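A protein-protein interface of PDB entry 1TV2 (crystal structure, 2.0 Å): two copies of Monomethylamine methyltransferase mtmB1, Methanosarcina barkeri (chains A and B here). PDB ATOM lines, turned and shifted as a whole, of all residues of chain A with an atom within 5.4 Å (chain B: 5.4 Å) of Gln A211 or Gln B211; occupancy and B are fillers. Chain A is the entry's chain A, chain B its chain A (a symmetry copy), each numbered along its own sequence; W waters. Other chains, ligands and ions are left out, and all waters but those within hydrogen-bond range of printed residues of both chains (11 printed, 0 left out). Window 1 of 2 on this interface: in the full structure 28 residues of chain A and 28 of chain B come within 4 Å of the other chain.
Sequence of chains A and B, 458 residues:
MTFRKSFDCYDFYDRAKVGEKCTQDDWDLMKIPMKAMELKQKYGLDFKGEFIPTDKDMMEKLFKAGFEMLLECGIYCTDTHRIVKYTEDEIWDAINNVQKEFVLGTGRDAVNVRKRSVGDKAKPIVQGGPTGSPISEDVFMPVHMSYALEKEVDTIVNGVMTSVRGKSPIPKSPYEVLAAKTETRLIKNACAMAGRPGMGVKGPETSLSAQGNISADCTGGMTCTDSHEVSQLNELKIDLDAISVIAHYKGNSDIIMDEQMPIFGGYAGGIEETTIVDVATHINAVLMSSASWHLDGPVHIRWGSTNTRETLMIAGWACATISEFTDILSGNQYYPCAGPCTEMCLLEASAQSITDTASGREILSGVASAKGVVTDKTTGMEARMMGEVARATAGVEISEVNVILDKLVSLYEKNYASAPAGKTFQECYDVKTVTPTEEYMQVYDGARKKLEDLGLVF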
ATOM      1  N   LYS A 172     -12.669 -14.707 -15.214  1.00  0.00           N
ATOM      2  CA  LYS A 172     -11.588 -15.677 -15.102  1.00  0.00           C
ATOM      3  C   LYS A 172     -10.664 -15.478 -13.905  1.00  0.00           C
ATOM      4  O   LYS A 172      -9.558 -16.015 -13.867  1.00  0.00           O
ATOM      5  CB  LYS A 172     -10.792 -15.742 -16.411  1.00  0.00           C
ATOM      6  CG  LYS A 172     -11.631 -16.310 -17.550  1.00  0.00           C
ATOM      7  CD  LYS A 172     -10.847 -16.526 -18.828  1.00  0.00           C
ATOM      8  CE  LYS A 172     -11.769 -17.062 -19.918  1.00  0.00           C
ATOM      9  NZ  LYS A 172     -11.084 -17.223 -21.234  1.00  0.00           N
ATOM     10  N   SER A 173     -11.128 -14.711 -12.922  1.00  0.00           N
ATOM     11  CA  SER A 173     -10.371 -14.496 -11.693  1.00  0.00           C
ATOM     12  C   SER A 173     -11.131 -15.301 -10.637  1.00  0.00           C
ATOM     13  O   SER A 173     -12.303 -15.632 -10.835  1.00  0.00           O
ATOM     14  CB  SER A 173     -10.375 -13.017 -11.295  1.00  0.00           C
ATOM     15  OG  SER A 173     -11.632 -12.642 -10.747  1.00  0.00           O
ATOM     16  N   GLU A 176     -14.538 -14.001  -9.644  1.00  0.00           N
ATOM     17  CA  GLU A 176     -15.708 -14.215 -10.491  1.00  0.00           C
ATOM     18  C   GLU A 176     -16.441 -15.467 -10.014  1.00  0.00           C
ATOM     19  O   GLU A 176     -17.671 -15.499  -9.981  1.00  0.00           O
ATOM     20  CB  GLU A 176     -15.315 -14.388 -11.964  1.00  0.00           C
ATOM     21  CG  GLU A 176     -16.509 -14.773 -12.843  1.00  0.00           C
ATOM     22  CD  GLU A 176     -16.142 -15.050 -14.289  1.00  0.00           C
ATOM     23  OE1 GLU A 176     -15.114 -15.719 -14.525  1.00  0.00           O
ATOM     24  OE2 GLU A 176     -16.896 -14.616 -15.185  1.00  0.00           O
ATOM     25  N   VAL A 177     -15.681 -16.499  -9.655  1.00  0.00           N
ATOM     26  CA  VAL A 177     -16.264 -17.744  -9.159  1.00  0.00           C
ATOM     27  C   VAL A 177     -16.970 -17.460  -7.835  1.00  0.00           C
ATOM     28  O   VAL A 177     -18.105 -17.889  -7.621  1.00  0.00           O
ATOM     29  CB  VAL A 177     -15.175 -18.829  -8.940  1.00  0.00           C
ATOM     30  CG1 VAL A 177     -15.724 -19.979  -8.104  1.00  0.00           C
ATOM     31  CG2 VAL A 177     -14.701 -19.358 -10.292  1.00  0.00           C
ATOM     32  N   SER A 209     -17.686 -15.381 -17.833  1.00  0.00           N
ATOM     33  CA  SER A 209     -16.968 -16.471 -18.482  1.00  0.00           C
ATOM     34  C   SER A 209     -17.714 -17.787 -18.280  1.00  0.00           C
ATOM     35  O   SER A 209     -18.594 -17.889 -17.424  1.00  0.00           O
ATOM     36  CB  SER A 209     -15.564 -16.608 -17.898  1.00  0.00           C
ATOM     37  OG  SER A 209     -15.613 -17.149 -16.590  1.00  0.00           O
ATOM     38  N   ALA A 210     -17.346 -18.793 -19.066  1.00  0.00           N
ATOM     39  CA  ALA A 210     -17.969 -20.105 -18.965  1.00  0.00           C
ATOM     40  C   ALA A 210     -17.689 -20.724 -17.595  1.00  0.00           C
ATOM     41  O   ALA A 210     -18.596 -21.255 -16.951  1.00  0.00           O
ATOM     42  CB  ALA A 210     -17.448 -21.019 -20.066  1.00  0.00           C
ATOM     43  N   GLN A 211     -16.436 -20.655 -17.149  1.00  0.00           N
ATOM     44  CA  GLN A 211     -16.077 -21.224 -15.853  1.00  0.00           C
ATOM     45  C   GLN A 211     -16.836 -20.515 -14.735  1.00  0.00           C
ATOM     46  O   GLN A 211     -17.259 -21.143 -13.763  1.00  0.00           O
ATOM     47  CB  GLN A 211     -14.562 -21.136 -15.621  1.00  0.00           C
ATOM     48  CG  GLN A 211     -13.999 -19.730 -15.488  1.00  0.00           C
ATOM     49  CD  GLN A 211     -12.496 -19.696 -15.700  1.00  0.00           C
ATOM     50  OE1 GLN A 211     -12.007 -20.077 -16.763  1.00  0.00           O
ATOM     51  NE2 GLN A 211     -11.756 -19.241 -14.691  1.00  0.00           N
ATOM     52  N   GLY A 212     -17.021 -19.206 -14.885  1.00  0.00           N
ATOM     53  CA  GLY A 212     -17.747 -18.449 -13.881  1.00  0.00           C
ATOM     54  C   GLY A 212     -19.192 -18.909 -13.771  1.00  0.00           C
ATOM     55  O   GLY A 212     -19.671 -19.219 -12.677  1.00  0.00           O
ATOM     56  N   ASN A 213     -19.886 -18.959 -14.905  1.00  0.00           N
ATOM     57  CA  ASN A 213     -21.281 -19.379 -14.926  1.00  0.00           C
ATOM     58  C   ASN A 213     -21.448 -20.820 -14.440  1.00  0.00           C
ATOM     59  O   ASN A 213     -22.380 -21.128 -13.699  1.00  0.00           O
ATOM     60  CB  ASN A 213     -21.862 -19.239 -16.340  1.00  0.00           C
ATOM     61  CG  ASN A 213     -21.856 -17.800 -16.834  1.00  0.00           C
ATOM     62  OD1 ASN A 213     -22.195 -16.882 -16.089  1.00  0.00           O
ATOM     63  ND2 ASN A 213     -21.479 -17.600 -18.099  1.00  0.00           N
ATOM     64  N   ILE A 214     -20.533 -21.692 -14.848  1.00  0.00           N
ATOM     65  CA  ILE A 214     -20.590 -23.099 -14.466  1.00  0.00           C
ATOM     66  C   ILE A 214     -20.413 -23.345 -12.964  1.00  0.00           C
ATOM     67  O   ILE A 214     -20.883 -24.351 -12.437  1.00  0.00           O
ATOM     68  CB  ILE A 214     -19.547 -23.910 -15.284  1.00  0.00           C
ATOM     69  CG1 ILE A 214     -19.975 -23.917 -16.757  1.00  0.00           C
ATOM     70  CG2 ILE A 214     -19.422 -25.345 -14.751  1.00  0.00           C
ATOM     71  CD1 ILE A 214     -19.000 -24.601 -17.697  1.00  0.00           C
ATOM     72  N   SER A 215     -19.763 -22.414 -12.270  1.00  0.00           N
ATOM     73  CA  SER A 215     -19.535 -22.557 -10.833  1.00  0.00           C
ATOM     74  C   SER A 215     -20.733 -22.116  -9.992  1.00  0.00           C
ATOM     75  O   SER A 215     -20.768 -22.359  -8.789  1.00  0.00           O
ATOM     76  CB  SER A 215     -18.323 -21.726 -10.407  1.00  0.00           C
ATOM     77  OG  SER A 215     -18.637 -20.340 -10.432  1.00  0.00           O
ATOM     78  N   ASP A 241     -18.301 -20.787 -25.717  1.00  0.00           N
ATOM     79  CA  ASP A 241     -18.428 -20.698 -24.263  1.00  0.00           C
ATOM     80  C   ASP A 241     -19.859 -21.045 -23.869  1.00  0.00           C
ATOM     81  O   ASP A 241     -20.092 -21.800 -22.923  1.00  0.00           O
ATOM     82  CB  ASP A 241     -18.105 -19.284 -23.784  1.00  0.00           C
ATOM     83  CG  ASP A 241     -16.680 -19.144 -23.302  1.00  0.00           C
ATOM     84  OD1 ASP A 241     -15.797 -19.878 -23.801  1.00  0.00           O
ATOM     85  OD2 ASP A 241     -16.444 -18.286 -22.425  1.00  0.00           O
ATOM     86  N   SER A 244     -20.666 -24.820 -24.079  1.00  0.00           N
ATOM     87  CA  SER A 244     -20.199 -25.605 -22.940  1.00  0.00           C
ATOM     88  C   SER A 244     -21.075 -25.372 -21.713  1.00  0.00           C
ATOM     89  O   SER A 244     -21.334 -26.297 -20.942  1.00  0.00           O
ATOM     90  CB  SER A 244     -18.746 -25.264 -22.604  1.00  0.00           C
ATOM     91  OG  SER A 244     -17.861 -25.926 -23.492  1.00  0.00           O
ATOM     92  N   LYS B 172     -12.396 -27.260 -23.389  1.00  0.00           N
ATOM     93  CA  LYS B 172     -13.287 -26.152 -23.708  1.00  0.00           C
ATOM     94  C   LYS B 172     -14.377 -26.472 -24.724  1.00  0.00           C
ATOM     95  O   LYS B 172     -14.981 -25.572 -25.304  1.00  0.00           O
ATOM     96  CB  LYS B 172     -12.476 -24.922 -24.133  1.00  0.00           C
ATOM     97  CG  LYS B 172     -11.652 -24.366 -22.978  1.00  0.00           C
ATOM     98  CD  LYS B 172     -10.945 -23.068 -23.311  1.00  0.00           C
ATOM     99  CE  LYS B 172     -10.122 -22.604 -22.113  1.00  0.00           C
ATOM    100  NZ  LYS B 172      -9.328 -21.372 -22.393  1.00  0.00           N
ATOM    101  N   SER B 173     -14.634 -27.761 -24.928  1.00  0.00           N
ATOM    102  CA  SER B 173     -15.699 -28.199 -25.825  1.00  0.00           C
ATOM    103  C   SER B 173     -16.784 -28.733 -24.888  1.00  0.00           C
ATOM    104  O   SER B 173     -16.502 -29.047 -23.729  1.00  0.00           O
ATOM    105  CB  SER B 173     -15.220 -29.335 -26.736  1.00  0.00           C
ATOM    106  OG  SER B 173     -15.135 -30.559 -26.018  1.00  0.00           O
ATOM    107  N   GLU B 176     -16.005 -31.938 -23.044  1.00  0.00           N
ATOM    108  CA  GLU B 176     -15.139 -31.944 -21.867  1.00  0.00           C
ATOM    109  C   GLU B 176     -16.008 -31.854 -20.615  1.00  0.00           C
ATOM    110  O   GLU B 176     -15.736 -32.515 -19.614  1.00  0.00           O
ATOM    111  CB  GLU B 176     -14.152 -30.771 -21.885  1.00  0.00           C
ATOM    112  CG  GLU B 176     -13.347 -30.669 -20.586  1.00  0.00           C
ATOM    113  CD  GLU B 176     -12.431 -29.460 -20.527  1.00  0.00           C
ATOM    114  OE1 GLU B 176     -12.866 -28.362 -20.931  1.00  0.00           O
ATOM    115  OE2 GLU B 176     -11.285 -29.610 -20.053  1.00  0.00           O
ATOM    116  N   VAL B 177     -17.048 -31.024 -20.672  1.00  0.00           N
ATOM    117  CA  VAL B 177     -17.967 -30.869 -19.546  1.00  0.00           C
ATOM    118  C   VAL B 177     -18.695 -32.192 -19.322  1.00  0.00           C
ATOM    119  O   VAL B 177     -18.806 -32.666 -18.190  1.00  0.00           O
ATOM    120  CB  VAL B 177     -19.006 -29.748 -19.818  1.00  0.00           C
ATOM    121  CG1 VAL B 177     -20.156 -29.828 -18.820  1.00  0.00           C
ATOM    122  CG2 VAL B 177     -18.329 -28.384 -19.711  1.00  0.00           C
ATOM    123  N   SER B 209      -9.368 -28.029 -18.622  1.00  0.00           N
ATOM    124  CA  SER B 209      -9.619 -26.600 -18.477  1.00  0.00           C
ATOM    125  C   SER B 209     -10.298 -26.317 -17.141  1.00  0.00           C
ATOM    126  O   SER B 209     -10.814 -27.228 -16.489  1.00  0.00           O
ATOM    127  CB  SER B 209     -10.522 -26.100 -19.602  1.00  0.00           C
ATOM    128  OG  SER B 209     -11.851 -26.557 -19.422  1.00  0.00           O
ATOM    129  N   ALA B 210     -10.304 -25.049 -16.745  1.00  0.00           N
ATOM    130  CA  ALA B 210     -10.932 -24.644 -15.495  1.00  0.00           C
ATOM    131  C   ALA B 210     -12.437 -24.913 -15.544  1.00  0.00           C
ATOM    132  O   ALA B 210     -13.007 -25.452 -14.592  1.00  0.00           O
ATOM    133  CB  ALA B 210     -10.675 -23.165 -15.235  1.00  0.00           C
ATOM    134  N   GLN B 211     -13.079 -24.538 -16.649  1.00  0.00           N
ATOM    135  CA  GLN B 211     -14.518 -24.752 -16.778  1.00  0.00           C
ATOM    136  C   GLN B 211     -14.838 -26.243 -16.731  1.00  0.00           C
ATOM    137  O   GLN B 211     -15.848 -26.655 -16.156  1.00  0.00           O
ATOM    138  CB  GLN B 211     -15.046 -24.124 -18.076  1.00  0.00           C
ATOM    139  CG  GLN B 211     -14.540 -24.757 -19.364  1.00  0.00           C
ATOM    140  CD  GLN B 211     -14.738 -23.844 -20.561  1.00  0.00           C
ATOM    141  OE1 GLN B 211     -14.216 -22.730 -20.590  1.00  0.00           O
ATOM    142  NE2 GLN B 211     -15.493 -24.309 -21.554  1.00  0.00           N
ATOM    143  N   GLY B 212     -13.965 -27.054 -17.324  1.00  0.00           N
ATOM    144  CA  GLY B 212     -14.176 -28.491 -17.316  1.00  0.00           C
ATOM    145  C   GLY B 212     -14.142 -29.052 -15.903  1.00  0.00           C
ATOM    146  O   GLY B 212     -15.062 -29.758 -15.486  1.00  0.00           O
ATOM    147  N   ASN B 213     -13.079 -28.736 -15.166  1.00  0.00           N
ATOM    148  CA  ASN B 213     -12.930 -29.220 -13.800  1.00  0.00           C
ATOM    149  C   ASN B 213     -14.054 -28.714 -12.893  1.00  0.00           C
ATOM    150  O   ASN B 213     -14.575 -29.460 -12.065  1.00  0.00           O
ATOM    151  CB  ASN B 213     -11.571 -28.795 -13.226  1.00  0.00           C
ATOM    152  CG  ASN B 213     -10.402 -29.382 -14.002  1.00  0.00           C
ATOM    153  OD1 ASN B 213     -10.418 -30.558 -14.364  1.00  0.00           O
ATOM    154  ND2 ASN B 213      -9.375 -28.565 -14.252  1.00  0.00           N
ATOM    155  N   ILE B 214     -14.431 -27.452 -13.065  1.00  0.00           N
ATOM    156  CA  ILE B 214     -15.481 -26.848 -12.252  1.00  0.00           C
ATOM    157  C   ILE B 214     -16.865 -27.476 -12.452  1.00  0.00           C
ATOM    158  O   ILE B 214     -17.708 -27.423 -11.559  1.00  0.00           O
ATOM    159  CB  ILE B 214     -15.530 -25.316 -12.508  1.00  0.00           C
ATOM    160  CG1 ILE B 214     -14.241 -24.686 -11.964  1.00  0.00           C
ATOM    161  CG2 ILE B 214     -16.763 -24.684 -11.844  1.00  0.00           C
ATOM    162  CD1 ILE B 214     -14.106 -23.196 -12.222  1.00  0.00           C
ATOM    163  N   SER B 215     -17.086 -28.096 -13.607  1.00  0.00           N
ATOM    164  CA  SER B 215     -18.375 -28.723 -13.899  1.00  0.00           C
ATOM    165  C   SER B 215     -18.504 -30.126 -13.306  1.00  0.00           C
ATOM    166  O   SER B 215     -19.592 -30.697 -13.297  1.00  0.00           O
ATOM    167  CB  SER B 215     -18.581 -28.825 -15.411  1.00  0.00           C
ATOM    168  OG  SER B 215     -17.733 -29.824 -15.963  1.00  0.00           O
ATOM    169  N   ASP B 241      -5.796 -20.479 -13.932  1.00  0.00           N
ATOM    170  CA  ASP B 241      -6.883 -21.448 -14.075  1.00  0.00           C
ATOM    171  C   ASP B 241      -7.018 -22.236 -12.778  1.00  0.00           C
ATOM    172  O   ASP B 241      -8.124 -22.452 -12.278  1.00  0.00           O
ATOM    173  CB  ASP B 241      -6.588 -22.413 -15.221  1.00  0.00           C
ATOM    174  CG  ASP B 241      -7.266 -22.012 -16.510  1.00  0.00           C
ATOM    175  OD1 ASP B 241      -7.488 -20.798 -16.725  1.00  0.00           O
ATOM    176  OD2 ASP B 241      -7.568 -22.918 -17.316  1.00  0.00           O
ATOM    177  N   SER B 244      -8.676 -20.248  -9.906  1.00  0.00           N
ATOM    178  CA  SER B 244     -10.132 -20.181  -9.976  1.00  0.00           C
ATOM    179  C   SER B 244     -10.766 -21.508  -9.572  1.00  0.00           C
ATOM    180  O   SER B 244     -11.816 -21.531  -8.929  1.00  0.00           O
ATOM    181  CB  SER B 244     -10.592 -19.801 -11.386  1.00  0.00           C
ATOM    182  OG  SER B 244     -10.463 -18.405 -11.592  1.00  0.00           O
HETATM  183  O   HOH W   1     -17.743 -25.311 -26.031  1.00  0.00           O
HETATM  184  O   HOH W   2     -20.181 -26.528 -11.043  1.00  0.00           O
HETATM  185  O   HOH W   3     -13.245 -17.413 -13.014  1.00  0.00           O
HETATM  186  O   HOH W   4      -8.125 -17.239 -11.705  1.00  0.00           O
HETATM  187  O   HOH W   5     -15.471 -27.202 -21.647  1.00  0.00           O
HETATM  188  O   HOH W   6     -11.965 -22.758 -18.754  1.00  0.00           O
HETATM  189  O   HOH W   7     -13.715 -20.428 -21.789  1.00  0.00           O
HETATM  190  O   HOH W   8     -15.746 -22.869 -24.104  1.00  0.00           O
HETATM  191  O   HOH W   9     -14.073 -19.915 -18.798  1.00  0.00           O
HETATM  192  O   HOH W  10      -9.934 -20.513 -18.343  1.00  0.00           O
HETATM  193  O   HOH W  11      -8.869 -18.772 -14.986  1.00  0.00           O
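Of the 13 printed residues of chain A, 8 touch a printed residue of chain B. Of the 13 printed residues of chain B, 8 touch a printed residue of chain A. Hydrophobic or aromatic side chains of chain B within 4 Å of the printed part of chain A: Val B177, Ala B210 and Ile B214. Among the printed residues, no Asp or Glu carboxylate lies within 4 Å of a Lys or Arg side-chain nitrogen of the other chain.
Ser A173 touches Ser B244, and with the chains exchanged Ser A244 touches Ser B173. Gln B211 touches its own counterpart, Gln A211. Gln A211 touches Ser B244, and with the chains exchanged Ser A244 touches Gln B211. Ile A214 touches its own counterpart, Ile B214. Of the 14 pairs that touch across the chains among the printed residues, 14 have their exchanged pair printed and touching as well.
Water W1 lies within hydrogen-bond range of OG of Ser A244 (2.6 Å) and O of Lys B172 (2.9 Å). Water W7 bridges OE1 of Gln B211 (2.6 Å) and OD1 of Asp A241 (2.9 Å). Water W9 lies within hydrogen-bond range of OE1 of Gln A211, OE1 of Gln B211 and N of Ala A210. Water W6 lies within hydrogen-bond range of OE1 of Gln B211 (2.9 Å), OE1 of Gln A211 (3.3 Å) and N of Ala B210 (3.5 Å). Water W8 lies within hydrogen-bond range of NE2 of Gln B211 (2.9 Å), OD1 of Asp A241 (3.0 Å) and O of Lys B172 (3.1 Å). Water W11 lies within hydrogen-bond range of the side-chain amide nitrogen (NE2) of Gln A211 (2.9 Å), the side-chain carboxylate (OD1) of Asp B241 (3.0 Å) and the backbone carbonyl oxygen (O) of Lys A172 (3.1 Å).
Among the printed residues, merely in contact across the chains: Val A177 with Ser B244 (3.9 Å), Ala A210 with Gln B211 (3.7 Å), Gln A211 with Ala B210 (3.7 Å), Gln A211 with Gln B211 (3.8 Å), Ile A214 with Ile B214 (3.99 Å), Ile A214 with Ser B215 (3.6 Å), Ser A215 with Ile B214 (3.6 Å) and Ser A244 with Val B177 (3.9 Å).
The side-chain carboxylate (OE1) of Glu A176 lies within hydrogen-bond range of the backbone NH (N) of Lys A172 (2.7 Å). OG of Ser A173 lies within hydrogen-bond range of N of Glu A176 (3.4 Å). The backbone carbonyl oxygen (O) of Gly A212 lies within hydrogen-bond range of the side-chain hydroxyl (OG) of Ser A215. The backbone NH (N) of Lys B172 sits at hydrogen-bond distance from the side-chain carboxylate (OE1) of Glu B176 (2.7 Å). The side-chain hydroxyl (OG) of Ser B173 sits at hydrogen-bond distance from the backbone NH (N) of Glu B176 (3.4 Å). The backbone carbonyl oxygen of Gly B212 sits at hydrogen-bond distance from the side-chain hydroxyl of Ser B215.
Of the printed residues of chain B, Val A177 touches Ser B244. Printed residues of chain B within 4 Å of Gln A211: Ala B210 (3.7 Å), Gln B211 (3.8 Å) and Ser B244 (3.5 Å). Of the printed residues of chain B, Ser A215 touches Ile B214 (3.6 Å). Of the printed residues of chain A, Lys B172 touches Ser A244. Printed residues of chain A within 4 Å of Gln B211: Ala A210 (3.7 Å), Gln A211 (3.8 Å) and Ser A244 (3.5 Å). Gly B212 touches none of the printed residues of chain A. Asn B213 touches none of the printed residues of chain A. The nearest printed residue of chain B that does not touch Gln A211 is Ile B214 (4.001 Å). The nearest printed residue of chain A that does not touch Gln B211 is Ile A214 (4.001 Å).
O of Lys A172 sits at hydrogen-bond distance from OG of Ser B244 (3.4 Å). The backbone carbonyl oxygen of Ser A173 sits close to the side-chain hydroxyl of Ser B244 (3.4 Å). The side-chain hydroxyl (OG) of Ser B244 sits at hydrogen-bond distance from the side-chain amide nitrogen (NE2) of Gln A211, at 3.5 Å. O of Lys B172 sits at hydrogen-bond distance from OG of Ser A244, at 3.4 Å. The side-chain hydroxyl (OG) of Ser A244 lies close to the backbone carbonyl oxygen (O) of Ser B173. The side-chain hydroxyl (OG) of Ser A244 sits at hydrogen-bond distance from the side-chain amide nitrogen (NE2) of Gln B211.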
